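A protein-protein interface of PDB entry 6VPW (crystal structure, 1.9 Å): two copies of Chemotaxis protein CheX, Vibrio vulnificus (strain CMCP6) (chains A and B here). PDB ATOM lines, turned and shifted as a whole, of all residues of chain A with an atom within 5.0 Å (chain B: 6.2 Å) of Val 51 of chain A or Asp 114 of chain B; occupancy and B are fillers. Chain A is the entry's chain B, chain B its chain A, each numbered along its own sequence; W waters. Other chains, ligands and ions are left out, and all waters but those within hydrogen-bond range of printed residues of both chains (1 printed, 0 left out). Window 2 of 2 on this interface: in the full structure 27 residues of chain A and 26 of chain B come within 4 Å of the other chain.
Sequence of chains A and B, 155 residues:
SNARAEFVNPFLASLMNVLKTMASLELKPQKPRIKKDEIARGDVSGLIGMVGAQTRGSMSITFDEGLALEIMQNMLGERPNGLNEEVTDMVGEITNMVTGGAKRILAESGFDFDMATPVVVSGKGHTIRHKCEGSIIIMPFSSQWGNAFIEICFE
Hydrophobic or aromatic side chains of chain A that line the printed part of chain B: Val 51.
Asp 114 of chain B touches just one residue of chain A: Val 51.
Of the printed residues of chain B, Met 50 of chain A touches Ala 116 (3.6 Å).
Of the printed residues of chain B, Asp 114 of chain A touches Val 51.
The nearest residue of chain B that does not touch Val 51 of chain A is Val 51 of chain B (4.4 Å).
Gly 49 of chain A touches Ala 116 of chain B (CA to CB, 3.5 Å).
Met 50 of chain A touches Ala 116 of chain B.
CB of Asp 114 of chain B touches CG1 of Val 51 of chain A, 3.96 Å away.
Met 115 of chain B touches Val 51 of chain A.
CG2 of Val 51 of chain A touches N of Ala 116 of chain B, at 3.9 Å.
O of Met 115 of chain B touches CD of Arg 56 of chain A, at 3.6 Å.
Gly 57 of chain A touches Ala 116 of chain B.
Val 51 of chain B touches Asp 114 of chain A.
Val 51 of chain A touches Asp 114 of chain B, and with the chains exchanged Asp 114 of chain A touches Val 51 of chain B.
Of the 8 pairs that touch across the chains among the printed residues, 2 have their exchanged pair printed and touching as well.
Water W1 bridges the backbone carbonyl oxygen of Met 115 of chain B (2.5 Å) and the guanidinium group of Arg 56 of chain A (3.0 Å).
The backbone NH (N) of Ala 116 of chain B sits at hydrogen-bond distance from the backbone carbonyl oxygen (O) of Gly 49 of chain B (2.9 Å).
O of Val 51 of chain B lies within hydrogen-bond range of N of Asp 114 of chain B, at 2.8 Å.
OD1 of Asp 114 of chain B lies within salt-bridge range of NZ of Lys 103 of chain B (3.6 Å).
The backbone carbonyl oxygen (O) of Gly 57 of chain A is in hydrogen-bond range of the backbone NH (N) of Met 50 of chain A (2.8 Å).
N of Asp 114 of chain A is in hydrogen-bond range of O of Val 51 of chain A.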
ATOM      1  N   GLY A  49     -29.084   9.219  34.734  1.00  0.00           N
ATOM      2  CA  GLY A  49     -28.453   9.289  33.409  1.00  0.00           C
ATOM      3  C   GLY A  49     -29.046  10.422  32.580  1.00  0.00           C
ATOM      4  O   GLY A  49     -30.220  10.778  32.793  1.00  0.00           O
ATOM      5  N   MET A  50     -28.283  10.911  31.601  1.00  0.00           N
ATOM      6  CA  MET A  50     -28.756  11.989  30.700  1.00  0.00           C
ATOM      7  C   MET A  50     -28.323  11.659  29.264  1.00  0.00           C
ATOM      8  O   MET A  50     -27.236  11.108  29.092  1.00  0.00           O
ATOM      9  CB  MET A  50     -28.173  13.339  31.137  1.00  0.00           C
ATOM     10  CG  MET A  50     -28.587  13.753  32.531  1.00  0.00           C
ATOM     11  SD  MET A  50     -27.579  15.137  33.150  1.00  0.00           S
ATOM     12  CE  MET A  50     -26.064  14.277  33.558  1.00  0.00           C
ATOM     13  N   VAL A  51     -29.183  11.954  28.289  1.00  0.00           N
ATOM     14  CA  VAL A  51     -28.884  11.693  26.851  1.00  0.00           C
ATOM     15  C   VAL A  51     -29.254  12.941  26.057  1.00  0.00           C
ATOM     16  O   VAL A  51     -30.392  13.448  26.231  1.00  0.00           O
ATOM     17  CB  VAL A  51     -29.645  10.465  26.322  1.00  0.00           C
ATOM     18  CG1 VAL A  51     -29.414  10.245  24.833  1.00  0.00           C
ATOM     19  CG2 VAL A  51     -29.295   9.211  27.094  1.00  0.00           C
ATOM     20  N   GLY A  52     -28.322  13.402  25.229  1.00  0.00           N
ATOM     21  CA  GLY A  52     -28.539  14.559  24.341  1.00  0.00           C
ATOM     22  C   GLY A  52     -28.086  14.234  22.932  1.00  0.00           C
ATOM     23  O   GLY A  52     -27.636  13.102  22.705  1.00  0.00           O
ATOM     24  N   ALA A  53     -28.201  15.185  22.010  1.00  0.00           N
ATOM     25  CA  ALA A  53     -27.777  14.939  20.614  1.00  0.00           C
ATOM     26  C   ALA A  53     -26.248  14.855  20.543  1.00  0.00           C
ATOM     27  O   ALA A  53     -25.735  13.850  20.017  1.00  0.00           O
ATOM     28  CB  ALA A  53     -28.303  16.030  19.717  1.00  0.00           C
ATOM     29  N   THR A  55     -24.099  14.771  23.159  1.00  0.00           N
ATOM     30  CA  THR A  55     -23.409  14.138  24.318  1.00  0.00           C
ATOM     31  C   THR A  55     -24.370  13.280  25.154  1.00  0.00           C
ATOM     32  O   THR A  55     -25.595  13.475  25.037  1.00  0.00           O
ATOM     33  CB  THR A  55     -22.772  15.229  25.191  1.00  0.00           C
ATOM     34  OG1 THR A  55     -22.022  14.620  26.243  1.00  0.00           O
ATOM     35  CG2 THR A  55     -23.796  16.182  25.772  1.00  0.00           C
ATOM     36  N   ARG A  56     -23.810  12.359  25.950  1.00  0.00           N
ATOM     37  CA  ARG A  56     -24.553  11.521  26.934  1.00  0.00           C
ATOM     38  C   ARG A  56     -23.731  11.442  28.222  1.00  0.00           C
ATOM     39  O   ARG A  56     -22.487  11.632  28.147  1.00  0.00           O
ATOM     40  CB  ARG A  56     -24.837  10.117  26.398  1.00  0.00           C
ATOM     41  CG  ARG A  56     -23.598   9.300  26.083  1.00  0.00           C
ATOM     42  CD  ARG A  56     -23.961   7.991  25.412  1.00  0.00           C
ATOM     43  NE  ARG A  56     -22.763   7.204  25.186  1.00  0.00           N
ATOM     44  CZ  ARG A  56     -22.741   5.988  24.661  1.00  0.00           C
ATOM     45  NH1 ARG A  56     -23.871   5.401  24.299  1.00  0.00           N
ATOM     46  NH2 ARG A  56     -21.586   5.362  24.506  1.00  0.00           N
ATOM     47  N   GLY A  57     -24.390  11.221  29.361  1.00  0.00           N
ATOM     48  CA  GLY A  57     -23.612  11.163  30.607  1.00  0.00           C
ATOM     49  C   GLY A  57     -24.435  10.816  31.831  1.00  0.00           C
ATOM     50  O   GLY A  57     -25.545  10.251  31.707  1.00  0.00           O
ATOM     51  N   PHE A 113     -30.183  18.199  26.863  1.00  0.00           N
ATOM     52  CA  PHE A 113     -30.195  16.766  27.216  1.00  0.00           C
ATOM     53  C   PHE A 113     -31.537  16.451  27.853  1.00  0.00           C
ATOM     54  O   PHE A 113     -32.233  17.372  28.343  1.00  0.00           O
ATOM     55  CB  PHE A 113     -29.043  16.402  28.156  1.00  0.00           C
ATOM     56  CG  PHE A 113     -29.112  17.037  29.519  1.00  0.00           C
ATOM     57  CD1 PHE A 113     -29.909  16.502  30.517  1.00  0.00           C
ATOM     58  CD2 PHE A 113     -28.366  18.171  29.808  1.00  0.00           C
ATOM     59  CE1 PHE A 113     -29.965  17.087  31.771  1.00  0.00           C
ATOM     60  CE2 PHE A 113     -28.426  18.752  31.063  1.00  0.00           C
ATOM     61  CZ  PHE A 113     -29.216  18.205  32.044  1.00  0.00           C
ATOM     62  N   ASP A 114     -31.890  15.176  27.779  1.00  0.00           N
ATOM     63  CA  ASP A 114     -33.102  14.624  28.415  1.00  0.00           C
ATOM     64  C   ASP A 114     -32.631  13.751  29.574  1.00  0.00           C
ATOM     65  O   ASP A 114     -31.601  13.071  29.440  1.00  0.00           O
ATOM     66  CB  ASP A 114     -33.950  13.859  27.409  1.00  0.00           C
ATOM     67  CG  ASP A 114     -34.462  14.735  26.284  1.00  0.00           C
ATOM     68  OD1 ASP A 114     -34.919  15.866  26.582  1.00  0.00           O
ATOM     69  OD2 ASP A 114     -34.349  14.299  25.130  1.00  0.00           O
ATOM     70  N   GLY B  49     -29.111   4.840  32.934  1.00  0.00           N
ATOM     71  CA  GLY B  49     -30.401   5.449  32.576  1.00  0.00           C
ATOM     72  C   GLY B  49     -30.690   5.224  31.110  1.00  0.00           C
ATOM     73  O   GLY B  49     -29.730   5.078  30.309  1.00  0.00           O
ATOM     74  N   MET B  50     -31.964   5.241  30.770  1.00  0.00           N
ATOM     75  CA  MET B  50     -32.389   5.048  29.368  1.00  0.00           C
ATOM     76  C   MET B  50     -33.459   6.080  29.031  1.00  0.00           C
ATOM     77  O   MET B  50     -34.392   6.272  29.861  1.00  0.00           O
ATOM     78  CB  MET B  50     -32.945   3.641  29.176  1.00  0.00           C
ATOM     79  CG  MET B  50     -31.858   2.581  29.273  1.00  0.00           C
ATOM     80  SD  MET B  50     -32.541   0.947  29.536  1.00  0.00           S
ATOM     81  CE  MET B  50     -33.032   1.067  31.254  1.00  0.00           C
ATOM     82  N   VAL B  51     -33.295   6.720  27.875  1.00  0.00           N
ATOM     83  CA  VAL B  51     -34.266   7.729  27.376  1.00  0.00           C
ATOM     84  C   VAL B  51     -34.634   7.386  25.931  1.00  0.00           C
ATOM     85  O   VAL B  51     -33.719   7.278  25.091  1.00  0.00           O
ATOM     86  CB  VAL B  51     -33.696   9.153  27.463  1.00  0.00           C
ATOM     87  CG1 VAL B  51     -34.647  10.189  26.856  1.00  0.00           C
ATOM     88  CG2 VAL B  51     -33.345   9.507  28.895  1.00  0.00           C
ATOM     89  N   GLY B  52     -35.931   7.231  25.685  1.00  0.00           N
ATOM     90  CA  GLY B  52     -36.466   7.037  24.327  1.00  0.00           C
ATOM     91  C   GLY B  52     -37.421   8.167  24.008  1.00  0.00           C
ATOM     92  O   GLY B  52     -37.634   9.016  24.905  1.00  0.00           O
ATOM     93  N   LYS B 103     -31.536  -3.422  24.232  1.00  0.00           N
ATOM     94  CA  LYS B 103     -31.901  -2.313  23.315  1.00  0.00           C
ATOM     95  C   LYS B 103     -32.076  -2.847  21.887  1.00  0.00           C
ATOM     96  O   LYS B 103     -33.026  -2.447  21.204  1.00  0.00           O
ATOM     97  CB  LYS B 103     -30.800  -1.249  23.325  1.00  0.00           C
ATOM     98  CG  LYS B 103     -30.955  -0.137  22.296  1.00  0.00           C
ATOM     99  CD  LYS B 103     -29.846   0.896  22.391  1.00  0.00           C
ATOM    100  CE  LYS B 103     -29.593   1.614  21.079  1.00  0.00           C
ATOM    101  NZ  LYS B 103     -30.739   2.427  20.650  1.00  0.00           N
ATOM    102  N   ASP B 112     -38.084   1.695  21.493  1.00  0.00           N
ATOM    103  CA  ASP B 112     -36.779   2.342  21.199  1.00  0.00           C
ATOM    104  C   ASP B 112     -36.273   3.174  22.378  1.00  0.00           C
ATOM    105  O   ASP B 112     -37.075   3.944  22.986  1.00  0.00           O
ATOM    106  CB  ASP B 112     -36.896   3.250  19.974  1.00  0.00           C
ATOM    107  CG  ASP B 112     -37.234   2.526  18.677  1.00  0.00           C
ATOM    108  OD1 ASP B 112     -36.475   1.626  18.288  1.00  0.00           O
ATOM    109  OD2 ASP B 112     -38.254   2.875  18.075  1.00  0.00           O
ATOM    110  N   PHE B 113     -34.972   3.078  22.649  1.00  0.00           N
ATOM    111  CA  PHE B 113     -34.371   3.945  23.695  1.00  0.00           C
ATOM    112  C   PHE B 113     -32.874   4.076  23.444  1.00  0.00           C
ATOM    113  O   PHE B 113     -32.291   3.217  22.742  1.00  0.00           O
ATOM    114  CB  PHE B 113     -34.656   3.414  25.104  1.00  0.00           C
ATOM    115  CG  PHE B 113     -34.051   2.072  25.422  1.00  0.00           C
ATOM    116  CD1 PHE B 113     -32.723   1.968  25.802  1.00  0.00           C
ATOM    117  CD2 PHE B 113     -34.813   0.914  25.345  1.00  0.00           C
ATOM    118  CE1 PHE B 113     -32.162   0.735  26.089  1.00  0.00           C
ATOM    119  CE2 PHE B 113     -34.261  -0.311  25.670  1.00  0.00           C
ATOM    120  CZ  PHE B 113     -32.930  -0.404  26.018  1.00  0.00           C
ATOM    121  N   ASP B 114     -32.292   5.144  23.992  1.00  0.00           N
ATOM    122  CA  ASP B 114     -30.829   5.390  23.948  1.00  0.00           C
ATOM    123  C   ASP B 114     -30.323   5.287  25.385  1.00  0.00           C
ATOM    124  O   ASP B 114     -31.119   5.605  26.302  1.00  0.00           O
ATOM    125  CB  ASP B 114     -30.518   6.748  23.326  1.00  0.00           C
ATOM    126  CG  ASP B 114     -30.967   6.848  21.883  1.00  0.00           C
ATOM    127  OD1 ASP B 114     -30.548   5.983  21.087  1.00  0.00           O
ATOM    128  OD2 ASP B 114     -31.768   7.759  21.590  1.00  0.00           O
ATOM    129  N   MET B 115     -29.081   4.842  25.573  1.00  0.00           N
ATOM    130  CA  MET B 115     -28.548   4.652  26.952  1.00  0.00           C
ATOM    131  C   MET B 115     -27.670   5.834  27.344  1.00  0.00           C
ATOM    132  O   MET B 115     -27.033   6.433  26.461  1.00  0.00           O
ATOM    133  CB  MET B 115     -27.650   3.417  27.059  1.00  0.00           C
ATOM    134  CG  MET B 115     -28.113   2.241  26.266  1.00  0.00           C
ATOM    135  SD  MET B 115     -26.760   1.042  26.181  1.00  0.00           S
ATOM    136  CE  MET B 115     -27.062   0.401  24.541  1.00  0.00           C
ATOM    137  N   ALA B 116     -27.623   6.088  28.639  1.00  0.00           N
ATOM    138  CA  ALA B 116     -26.718   7.085  29.229  1.00  0.00           C
ATOM    139  C   ALA B 116     -25.391   6.356  29.491  1.00  0.00           C
ATOM    140  O   ALA B 116     -25.127   5.363  28.813  1.00  0.00           O
ATOM    141  CB  ALA B 116     -27.331   7.643  30.482  1.00  0.00           C
HETATM  142  O   HOH W   1     -26.573   6.663  23.966  1.00  0.00           O
